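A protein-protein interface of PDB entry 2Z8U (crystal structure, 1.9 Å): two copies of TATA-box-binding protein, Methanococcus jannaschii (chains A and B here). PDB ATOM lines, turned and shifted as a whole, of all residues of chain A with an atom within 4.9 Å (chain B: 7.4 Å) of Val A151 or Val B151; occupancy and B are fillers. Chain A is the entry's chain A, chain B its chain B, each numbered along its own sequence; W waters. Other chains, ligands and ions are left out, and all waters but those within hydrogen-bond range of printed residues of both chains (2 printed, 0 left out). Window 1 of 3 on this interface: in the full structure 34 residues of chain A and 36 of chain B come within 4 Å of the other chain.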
ATOM      1  N   VAL A 142      13.198 -20.521 -22.772  1.00  0.00           N
ATOM      2  CA  VAL A 142      13.464 -19.188 -22.228  1.00  0.00           C
ATOM      3  C   VAL A 142      14.204 -19.369 -20.913  1.00  0.00           C
ATOM      4  O   VAL A 142      13.752 -20.111 -20.042  1.00  0.00           O
ATOM      5  CB  VAL A 142      12.168 -18.375 -22.006  1.00  0.00           C
ATOM      6  CG1 VAL A 142      12.481 -16.930 -21.539  1.00  0.00           C
ATOM      7  CG2 VAL A 142      11.334 -18.358 -23.276  1.00  0.00           C
ATOM      8  N   TYR A 143      15.346 -18.700 -20.798  1.00  0.00           N
ATOM      9  CA  TYR A 143      16.167 -18.740 -19.595  1.00  0.00           C
ATOM     10  C   TYR A 143      16.498 -17.326 -19.090  1.00  0.00           C
ATOM     11  O   TYR A 143      17.187 -16.547 -19.760  1.00  0.00           O
ATOM     12  CB  TYR A 143      17.448 -19.517 -19.854  1.00  0.00           C
ATOM     13  CG  TYR A 143      18.298 -19.784 -18.618  1.00  0.00           C
ATOM     14  CD1 TYR A 143      17.726 -19.910 -17.343  1.00  0.00           C
ATOM     15  CD2 TYR A 143      19.661 -19.968 -18.736  1.00  0.00           C
ATOM     16  CE1 TYR A 143      18.532 -20.186 -16.208  1.00  0.00           C
ATOM     17  CE2 TYR A 143      20.468 -20.254 -17.611  1.00  0.00           C
ATOM     18  CZ  TYR A 143      19.904 -20.346 -16.365  1.00  0.00           C
ATOM     19  OH  TYR A 143      20.717 -20.638 -15.271  1.00  0.00           O
ATOM     20  N   ARG A 144      16.020 -17.023 -17.898  1.00  0.00           N
ATOM     21  CA  ARG A 144      16.258 -15.740 -17.243  1.00  0.00           C
ATOM     22  C   ARG A 144      17.468 -15.845 -16.318  1.00  0.00           C
ATOM     23  O   ARG A 144      17.542 -16.769 -15.494  1.00  0.00           O
ATOM     24  CB  ARG A 144      15.009 -15.392 -16.452  1.00  0.00           C
ATOM     25  CG  ARG A 144      14.976 -14.039 -15.766  1.00  0.00           C
ATOM     26  CD  ARG A 144      13.531 -13.672 -15.474  1.00  0.00           C
ATOM     27  NE  ARG A 144      12.913 -14.456 -14.391  1.00  0.00           N
ATOM     28  CZ  ARG A 144      11.620 -14.380 -14.054  1.00  0.00           C
ATOM     29  NH1 ARG A 144      10.800 -13.578 -14.721  1.00  0.00           N
ATOM     30  NH2 ARG A 144      11.134 -15.109 -13.049  1.00  0.00           N
ATOM     31  N   LYS A 149      21.699  -9.373 -15.771  1.00  0.00           N
ATOM     32  CA  LYS A 149      20.253  -9.490 -15.841  1.00  0.00           C
ATOM     33  C   LYS A 149      19.897  -9.556 -17.338  1.00  0.00           C
ATOM     34  O   LYS A 149      19.814  -8.528 -18.030  1.00  0.00           O
ATOM     35  CB  LYS A 149      19.585  -8.307 -15.126  1.00  0.00           C
ATOM     36  CG  LYS A 149      18.058  -8.333 -15.137  1.00  0.00           C
ATOM     37  CD  LYS A 149      17.507  -6.962 -14.783  1.00  0.00           C
ATOM     38  CE  LYS A 149      16.023  -6.855 -15.084  1.00  0.00           C
ATOM     39  NZ  LYS A 149      15.649  -5.423 -14.967  1.00  0.00           N
ATOM     40  N   VAL A 150      19.752 -10.782 -17.827  1.00  0.00           N
ATOM     41  CA  VAL A 150      19.483 -11.020 -19.236  1.00  0.00           C
ATOM     42  C   VAL A 150      18.370 -12.043 -19.403  1.00  0.00           C
ATOM     43  O   VAL A 150      17.989 -12.739 -18.439  1.00  0.00           O
ATOM     44  CB  VAL A 150      20.751 -11.490 -20.039  1.00  0.00           C
ATOM     45  CG1 VAL A 150      21.854 -10.438 -19.985  1.00  0.00           C
ATOM     46  CG2 VAL A 150      21.276 -12.855 -19.550  1.00  0.00           C
ATOM     47  N   VAL A 151      17.854 -12.098 -20.630  1.00  0.00           N
ATOM     48  CA  VAL A 151      16.874 -13.105 -21.020  1.00  0.00           C
ATOM     49  C   VAL A 151      17.558 -13.876 -22.119  1.00  0.00           C
ATOM     50  O   VAL A 151      18.077 -13.288 -23.069  1.00  0.00           O
ATOM     51  CB  VAL A 151      15.563 -12.511 -21.576  1.00  0.00           C
ATOM     52  CG1 VAL A 151      14.635 -13.646 -22.006  1.00  0.00           C
ATOM     53  CG2 VAL A 151      14.867 -11.588 -20.553  1.00  0.00           C
ATOM     54  N   VAL A 152      17.604 -15.188 -21.972  1.00  0.00           N
ATOM     55  CA  VAL A 152      18.286 -16.026 -22.957  1.00  0.00           C
ATOM     56  C   VAL A 152      17.253 -16.908 -23.632  1.00  0.00           C
ATOM     57  O   VAL A 152      16.400 -17.479 -22.954  1.00  0.00           O
ATOM     58  CB  VAL A 152      19.315 -16.958 -22.290  1.00  0.00           C
ATOM     59  CG1 VAL A 152      20.087 -17.739 -23.348  1.00  0.00           C
ATOM     60  CG2 VAL A 152      20.262 -16.151 -21.433  1.00  0.00           C
ATOM     61  N   LEU A 153      17.320 -16.999 -24.957  1.00  0.00           N
ATOM     62  CA  LEU A 153      16.534 -17.978 -25.705  1.00  0.00           C
ATOM     63  C   LEU A 153      17.510 -19.040 -26.193  1.00  0.00           C
ATOM     64  O   LEU A 153      18.506 -18.713 -26.835  1.00  0.00           O
ATOM     65  CB  LEU A 153      15.822 -17.310 -26.893  1.00  0.00           C
ATOM     66  CG  LEU A 153      15.101 -15.982 -26.547  1.00  0.00           C
ATOM     67  CD1 LEU A 153      14.622 -15.216 -27.784  1.00  0.00           C
ATOM     68  CD2 LEU A 153      13.955 -16.180 -25.583  1.00  0.00           C
ATOM     69  N   VAL A 161      20.227 -16.884 -28.139  1.00  0.00           N
ATOM     70  CA  VAL A 161      20.029 -15.449 -28.322  1.00  0.00           C
ATOM     71  C   VAL A 161      19.985 -14.838 -26.934  1.00  0.00           C
ATOM     72  O   VAL A 161      19.201 -15.268 -26.078  1.00  0.00           O
ATOM     73  CB  VAL A 161      18.722 -15.116 -29.112  1.00  0.00           C
ATOM     74  CG1 VAL A 161      18.574 -13.617 -29.314  1.00  0.00           C
ATOM     75  CG2 VAL A 161      18.731 -15.796 -30.455  1.00  0.00           C
ATOM     76  N   ILE A 162      20.843 -13.846 -26.711  1.00  0.00           N
ATOM     77  CA  ILE A 162      20.912 -13.176 -25.416  1.00  0.00           C
ATOM     78  C   ILE A 162      20.415 -11.742 -25.584  1.00  0.00           C
ATOM     79  O   ILE A 162      20.882 -11.012 -26.454  1.00  0.00           O
ATOM     80  CB  ILE A 162      22.351 -13.231 -24.828  1.00  0.00           C
ATOM     81  CG1 ILE A 162      22.883 -14.674 -24.852  1.00  0.00           C
ATOM     82  CG2 ILE A 162      22.374 -12.673 -23.387  1.00  0.00           C
ATOM     83  CD1 ILE A 162      24.403 -14.763 -24.713  1.00  0.00           C
ATOM     84  N   THR A 163      19.425 -11.361 -24.774  1.00  0.00           N
ATOM     85  CA  THR A 163      18.829 -10.044 -24.836  1.00  0.00           C
ATOM     86  C   THR A 163      18.842  -9.406 -23.437  1.00  0.00           C
ATOM     87  O   THR A 163      19.018 -10.094 -22.435  1.00  0.00           O
ATOM     88  CB  THR A 163      17.347 -10.129 -25.376  1.00  0.00           C
ATOM     89  OG1 THR A 163      16.498 -10.683 -24.371  1.00  0.00           O
ATOM     90  CG2 THR A 163      17.238 -11.033 -26.606  1.00  0.00           C
ATOM     91  N   MET B 109       5.179 -20.438 -14.150  1.00  0.00           N
ATOM     92  CA  MET B 109       3.978 -20.725 -14.950  1.00  0.00           C
ATOM     93  C   MET B 109       4.133 -20.095 -16.312  1.00  0.00           C
ATOM     94  O   MET B 109       4.784 -19.058 -16.448  1.00  0.00           O
ATOM     95  CB  MET B 109       2.710 -20.129 -14.330  1.00  0.00           C
ATOM     96  CG  MET B 109       2.547 -20.274 -12.838  1.00  0.00           C
ATOM     97  SD  MET B 109       1.162 -19.357 -12.118  1.00  0.00           S
ATOM     98  CE  MET B 109      -0.151 -20.532 -12.364  1.00  0.00           C
ATOM     99  N   ALA B 111       1.640 -18.462 -19.015  1.00  0.00           N
ATOM    100  CA  ALA B 111       0.290 -17.982 -19.265  1.00  0.00           C
ATOM    101  C   ALA B 111       0.279 -17.431 -20.686  1.00  0.00           C
ATOM    102  O   ALA B 111       1.292 -16.885 -21.176  1.00  0.00           O
ATOM    103  CB  ALA B 111      -0.077 -16.898 -18.299  1.00  0.00           C
ATOM    104  N   GLY B 130      13.102  -1.531 -22.705  1.00  0.00           N
ATOM    105  CA  GLY B 130      13.301  -2.909 -22.262  1.00  0.00           C
ATOM    106  C   GLY B 130      12.670  -3.946 -23.179  1.00  0.00           C
ATOM    107  O   GLY B 130      12.293  -5.046 -22.725  1.00  0.00           O
ATOM    108  N   LEU B 141       8.520 -10.364 -30.073  1.00  0.00           N
ATOM    109  CA  LEU B 141       9.206  -9.330 -29.346  1.00  0.00           C
ATOM    110  C   LEU B 141       9.342  -9.731 -27.859  1.00  0.00           C
ATOM    111  O   LEU B 141       8.380 -10.240 -27.251  1.00  0.00           O
ATOM    112  CB  LEU B 141       8.392  -8.046 -29.477  1.00  0.00           C
ATOM    113  CG  LEU B 141       8.873  -6.798 -28.753  1.00  0.00           C
ATOM    114  CD1 LEU B 141       8.636  -5.599 -29.619  1.00  0.00           C
ATOM    115  CD2 LEU B 141       8.166  -6.656 -27.423  1.00  0.00           C
ATOM    116  N   VAL B 142      10.528  -9.501 -27.292  1.00  0.00           N
ATOM    117  CA  VAL B 142      10.811  -9.833 -25.895  1.00  0.00           C
ATOM    118  C   VAL B 142      10.697  -8.580 -25.033  1.00  0.00           C
ATOM    119  O   VAL B 142      11.256  -7.528 -25.333  1.00  0.00           O
ATOM    120  CB  VAL B 142      12.189 -10.529 -25.715  1.00  0.00           C
ATOM    121  CG1 VAL B 142      12.425 -10.919 -24.255  1.00  0.00           C
ATOM    122  CG2 VAL B 142      12.276 -11.773 -26.609  1.00  0.00           C
ATOM    123  N   TYR B 143       9.947  -8.717 -23.951  1.00  0.00           N
ATOM    124  CA  TYR B 143       9.629  -7.606 -23.095  1.00  0.00           C
ATOM    125  C   TYR B 143       9.766  -8.083 -21.649  1.00  0.00           C
ATOM    126  O   TYR B 143       9.049  -8.972 -21.215  1.00  0.00           O
ATOM    127  CB  TYR B 143       8.187  -7.193 -23.418  1.00  0.00           C
ATOM    128  CG  TYR B 143       7.620  -6.017 -22.673  1.00  0.00           C
ATOM    129  CD1 TYR B 143       6.241  -5.920 -22.461  1.00  0.00           C
ATOM    130  CD2 TYR B 143       8.437  -5.003 -22.184  1.00  0.00           C
ATOM    131  CE1 TYR B 143       5.697  -4.837 -21.791  1.00  0.00           C
ATOM    132  CE2 TYR B 143       7.903  -3.919 -21.515  1.00  0.00           C
ATOM    133  CZ  TYR B 143       6.533  -3.842 -21.329  1.00  0.00           C
ATOM    134  OH  TYR B 143       5.997  -2.765 -20.661  1.00  0.00           O
ATOM    135  N   ARG B 144      10.691  -7.506 -20.904  1.00  0.00           N
ATOM    136  CA  ARG B 144      10.845  -7.894 -19.507  1.00  0.00           C
ATOM    137  C   ARG B 144      10.107  -6.928 -18.574  1.00  0.00           C
ATOM    138  O   ARG B 144      10.243  -5.707 -18.708  1.00  0.00           O
ATOM    139  CB  ARG B 144      12.333  -8.025 -19.153  1.00  0.00           C
ATOM    140  CG  ARG B 144      12.594  -8.729 -17.826  1.00  0.00           C
ATOM    141  CD  ARG B 144      13.989  -9.314 -17.806  1.00  0.00           C
ATOM    142  NE  ARG B 144      14.382  -9.866 -16.506  1.00  0.00           N
ATOM    143  CZ  ARG B 144      15.522 -10.521 -16.289  1.00  0.00           C
ATOM    144  NH1 ARG B 144      16.373 -10.708 -17.288  1.00  0.00           N
ATOM    145  NH2 ARG B 144      15.831 -10.974 -15.064  1.00  0.00           N
ATOM    146  N   LEU B 145       9.317  -7.462 -17.642  1.00  0.00           N
ATOM    147  CA  LEU B 145       8.672  -6.628 -16.617  1.00  0.00           C
ATOM    148  C   LEU B 145       9.343  -6.810 -15.255  1.00  0.00           C
ATOM    149  O   LEU B 145       9.840  -7.892 -14.944  1.00  0.00           O
ATOM    150  CB  LEU B 145       7.177  -6.944 -16.496  1.00  0.00           C
ATOM    151  CG  LEU B 145       6.174  -6.582 -17.598  1.00  0.00           C
ATOM    152  CD1 LEU B 145       4.745  -6.855 -17.098  1.00  0.00           C
ATOM    153  CD2 LEU B 145       6.319  -5.128 -18.022  1.00  0.00           C
ATOM    154  N   PRO B 148       4.803  -7.561 -12.127  1.00  0.00           N
ATOM    155  CA  PRO B 148       5.538  -8.667 -11.525  1.00  0.00           C
ATOM    156  C   PRO B 148       6.797  -8.964 -12.329  1.00  0.00           C
ATOM    157  O   PRO B 148       6.929  -8.512 -13.477  1.00  0.00           O
ATOM    158  CB  PRO B 148       4.545  -9.840 -11.598  1.00  0.00           C
ATOM    159  CG  PRO B 148       3.639  -9.506 -12.712  1.00  0.00           C
ATOM    160  CD  PRO B 148       3.531  -8.002 -12.732  1.00  0.00           C
ATOM    161  N   LYS B 149       7.724  -9.689 -11.719  1.00  0.00           N
ATOM    162  CA  LYS B 149       8.985 -10.033 -12.374  1.00  0.00           C
ATOM    163  C   LYS B 149       8.720 -11.151 -13.367  1.00  0.00           C
ATOM    164  O   LYS B 149       8.727 -12.329 -13.005  1.00  0.00           O
ATOM    165  CB  LYS B 149      10.020 -10.453 -11.330  1.00  0.00           C
ATOM    166  CG  LYS B 149      11.338 -10.947 -11.908  1.00  0.00           C
ATOM    167  CD  LYS B 149      12.212 -11.556 -10.806  1.00  0.00           C
ATOM    168  CE  LYS B 149      13.453 -12.209 -11.419  1.00  0.00           C
ATOM    169  NZ  LYS B 149      14.204 -12.988 -10.389  1.00  0.00           N
ATOM    170  N   VAL B 150       8.444 -10.771 -14.615  1.00  0.00           N
ATOM    171  CA  VAL B 150       8.081 -11.733 -15.658  1.00  0.00           C
ATOM    172  C   VAL B 150       8.790 -11.427 -16.973  1.00  0.00           C
ATOM    173  O   VAL B 150       9.297 -10.330 -17.172  1.00  0.00           O
ATOM    174  CB  VAL B 150       6.553 -11.792 -15.893  1.00  0.00           C
ATOM    175  CG1 VAL B 150       5.841 -12.297 -14.624  1.00  0.00           C
ATOM    176  CG2 VAL B 150       6.009 -10.449 -16.314  1.00  0.00           C
ATOM    177  N   VAL B 151       8.819 -12.414 -17.861  1.00  0.00           N
ATOM    178  CA  VAL B 151       9.304 -12.230 -19.215  1.00  0.00           C
ATOM    179  C   VAL B 151       8.128 -12.418 -20.113  1.00  0.00           C
ATOM    180  O   VAL B 151       7.394 -13.405 -19.989  1.00  0.00           O
ATOM    181  CB  VAL B 151      10.436 -13.227 -19.593  1.00  0.00           C
ATOM    182  CG1 VAL B 151      10.773 -13.129 -21.115  1.00  0.00           C
ATOM    183  CG2 VAL B 151      11.642 -12.934 -18.767  1.00  0.00           C
ATOM    184  N   VAL B 152       7.917 -11.452 -21.001  1.00  0.00           N
ATOM    185  CA  VAL B 152       6.761 -11.484 -21.910  1.00  0.00           C
ATOM    186  C   VAL B 152       7.254 -11.626 -23.351  1.00  0.00           C
ATOM    187  O   VAL B 152       8.244 -11.010 -23.725  1.00  0.00           O
ATOM    188  CB  VAL B 152       5.908 -10.202 -21.779  1.00  0.00           C
ATOM    189  CG1 VAL B 152       4.666 -10.267 -22.701  1.00  0.00           C
ATOM    190  CG2 VAL B 152       5.474  -9.988 -20.309  1.00  0.00           C
ATOM    191  N   LEU B 153       6.599 -12.481 -24.118  1.00  0.00           N
ATOM    192  CA  LEU B 153       6.834 -12.559 -25.553  1.00  0.00           C
ATOM    193  C   LEU B 153       5.548 -12.179 -26.265  1.00  0.00           C
ATOM    194  O   LEU B 153       4.472 -12.714 -25.963  1.00  0.00           O
ATOM    195  CB  LEU B 153       7.258 -13.965 -25.971  1.00  0.00           C
ATOM    196  CG  LEU B 153       8.206 -14.717 -25.031  1.00  0.00           C
ATOM    197  CD1 LEU B 153       8.274 -16.170 -25.455  1.00  0.00           C
ATOM    198  CD2 LEU B 153       9.587 -14.085 -25.045  1.00  0.00           C
ATOM    199  N   VAL B 160       0.263 -13.471 -26.796  1.00  0.00           N
ATOM    200  CA  VAL B 160       1.196 -12.992 -25.770  1.00  0.00           C
ATOM    201  C   VAL B 160       1.468 -14.194 -24.876  1.00  0.00           C
ATOM    202  O   VAL B 160       0.532 -14.926 -24.509  1.00  0.00           O
ATOM    203  CB  VAL B 160       0.534 -11.887 -24.906  1.00  0.00           C
ATOM    204  CG1 VAL B 160       1.394 -11.529 -23.714  1.00  0.00           C
ATOM    205  CG2 VAL B 160       0.258 -10.652 -25.741  1.00  0.00           C
ATOM    206  N   VAL B 161       2.729 -14.402 -24.527  1.00  0.00           N
ATOM    207  CA  VAL B 161       3.083 -15.482 -23.609  1.00  0.00           C
ATOM    208  C   VAL B 161       3.775 -14.798 -22.449  1.00  0.00           C
ATOM    209  O   VAL B 161       4.712 -14.014 -22.650  1.00  0.00           O
ATOM    210  CB  VAL B 161       4.049 -16.500 -24.268  1.00  0.00           C
ATOM    211  CG1 VAL B 161       4.583 -17.537 -23.241  1.00  0.00           C
ATOM    212  CG2 VAL B 161       3.397 -17.177 -25.469  1.00  0.00           C
ATOM    213  N   ILE B 162       3.335 -15.096 -21.231  1.00  0.00           N
ATOM    214  CA  ILE B 162       3.981 -14.543 -20.048  1.00  0.00           C
ATOM    215  C   ILE B 162       4.651 -15.682 -19.271  1.00  0.00           C
ATOM    216  O   ILE B 162       4.000 -16.695 -18.997  1.00  0.00           O
ATOM    217  CB  ILE B 162       2.960 -13.801 -19.163  1.00  0.00           C
ATOM    218  CG1 ILE B 162       2.189 -12.753 -19.993  1.00  0.00           C
ATOM    219  CG2 ILE B 162       3.655 -13.138 -17.985  1.00  0.00           C
ATOM    220  CD1 ILE B 162       0.938 -12.233 -19.316  1.00  0.00           C
ATOM    221  N   THR B 163       5.944 -15.533 -18.952  1.00  0.00           N
ATOM    222  CA  THR B 163       6.683 -16.571 -18.208  1.00  0.00           C
ATOM    223  C   THR B 163       7.313 -15.994 -16.949  1.00  0.00           C
ATOM    224  O   THR B 163       7.384 -14.775 -16.785  1.00  0.00           O
ATOM    225  CB  THR B 163       7.751 -17.284 -19.086  1.00  0.00           C
ATOM    226  OG1 THR B 163       8.825 -16.383 -19.393  1.00  0.00           O
ATOM    227  CG2 THR B 163       7.158 -17.757 -20.416  1.00  0.00           C
ATOM    228  N   GLY B 164       7.768 -16.855 -16.043  1.00  0.00           N
ATOM    229  CA  GLY B 164       8.381 -16.382 -14.810  1.00  0.00           C
ATOM    230  C   GLY B 164       7.377 -16.102 -13.709  1.00  0.00           C
ATOM    231  O   GLY B 164       7.735 -15.618 -12.631  1.00  0.00           O
ATOM    232  N   LEU B 165       6.121 -16.442 -13.972  1.00  0.00           N
ATOM    233  CA  LEU B 165       5.010 -16.210 -13.046  1.00  0.00           C
ATOM    234  C   LEU B 165       4.999 -17.080 -11.801  1.00  0.00           C
ATOM    235  O   LEU B 165       5.268 -18.269 -11.881  1.00  0.00           O
ATOM    236  CB  LEU B 165       3.701 -16.463 -13.771  1.00  0.00           C
ATOM    237  CG  LEU B 165       3.310 -15.391 -14.771  1.00  0.00           C
ATOM    238  CD1 LEU B 165       2.336 -15.967 -15.778  1.00  0.00           C
ATOM    239  CD2 LEU B 165       2.724 -14.221 -14.020  1.00  0.00           C
ATOM    240  N   ILE B 178       0.828  -5.079 -19.914  1.00  0.00           N
ATOM    241  CA  ILE B 178       1.101  -5.290 -21.345  1.00  0.00           C
ATOM    242  C   ILE B 178       0.061  -4.539 -22.207  1.00  0.00           C
ATOM    243  O   ILE B 178       0.416  -3.745 -23.076  1.00  0.00           O
ATOM    244  CB  ILE B 178       1.131  -6.782 -21.673  1.00  0.00           C
ATOM    245  CG1 ILE B 178       2.296  -7.448 -20.929  1.00  0.00           C
ATOM    246  CG2 ILE B 178       1.220  -7.026 -23.179  1.00  0.00           C
ATOM    247  CD1 ILE B 178       2.083  -8.930 -20.634  1.00  0.00           C
HETATM  248  O   HOH W   1      16.867  -8.669 -19.048  1.00  0.00           O
HETATM  249  O   HOH W   2      11.774 -11.060 -15.440  1.00  0.00           O
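The guanidinium group of Arg A144 lies within hydrogen-bond range of the backbone carbonyl oxygen of Lys B149, 3.0 Å away.
The backbone carbonyl oxygen (O) of Gly B164 is in hydrogen-bond range of the guanidinium group (NH2) of Arg A144, at 3.5 Å.
The backbone carbonyl oxygen of Val A150 is in hydrogen-bond range of the guanidinium group of Arg B144, 2.8 Å away.
The backbone carbonyl oxygen of Gly B130 lies within hydrogen-bond range of the backbone NH of Arg B144 (3.5 Å).
O of Val A151 lies within hydrogen-bond range of N of Thr A163.
The backbone NH (N) of Leu B145 sits at hydrogen-bond distance from the backbone carbonyl oxygen (O) of Val B150 (2.9 Å).
The backbone NH (N) of Thr B163 lies within hydrogen-bond range of the backbone carbonyl oxygen (O) of Val B151 (2.8 Å).
Among the printed residues, merely in contact across the chains: Arg A144 with Arg B144 (3.3 Å), Arg A144 with Val B150 (3.4 Å), Arg A144 with Val B151 (3.9 Å), Lys A149 with Arg B144 (3.5 Å), Val A151 with Arg B144 (3.7 Å) and Val A151 with Val B151 (3.9 Å).
Of chain B, only Arg B144 and Val B151 come within 4 Å of Val A151.
Val B151 touches just these residues of chain A: Arg A144 and Val A151.
Printed residues of chain B within 4 Å of Arg A144: Arg B144 (3.3 Å), Lys B149 (3.0 Å), Val B150 (3.4 Å), Val B151 (3.9 Å) and Gly B164 (3.5 Å).
Printed residues of chain A within 4 Å of Val B150: Arg A144 (3.4 Å).
Printed residues of chain B within 4 Å of Lys A149: Arg B144 (3.5 Å).
Val B152 touches none of the printed residues of chain A.
The nearest residue of chain B that does not touch Val A151 is Val B142 (4.2 Å).
The nearest printed residue of chain B that does not touch Val A150 is Val B151 (6.4 Å).
Printed residues of chain B that touch a printed residue of chain A: Arg B144, Lys B149, Val B150, Val B151 and Gly B164.
Of the 11 printed residues of chain A, 4 touch a printed residue of chain B.
Printed residues of chain A that touch a printed residue of chain B: Arg A144, Lys A149, Val A150 and Val A151.
Hydrophobic or aromatic side chains of chain A that line the printed part of chain B: Val A151.
Among the printed residues, 9 pairs touch across the chains.
Among the printed residues, no Asp or Glu carboxylate lies within 4 Å of a Lys or Arg side-chain nitrogen of the other chain.
Arg A144 touches its own counterpart, Arg B144.
Arg A144 touches Lys B149, and with the chains exchanged Lys A149 touches Arg B144.
Arg A144 touches Val B150, and with the chains exchanged Val A150 touches Arg B144.
Val B151 touches its own counterpart, Val A151.
Positions printed for both chains: 142, 143, 144, 149, 150, 151, 152, 153, 161, 162 and 163.
Water W1 bridges the guanidinium group (NH1) of Arg B144 and the backbone carbonyl oxygen (O) of Lys A149.
Water W2 lies within hydrogen-bond range of the guanidinium group of Arg A144 (2.8 Å), the guanidinium group of Arg B144 (3.1 Å) and the backbone carbonyl oxygen of Val B150 (3.1 Å).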
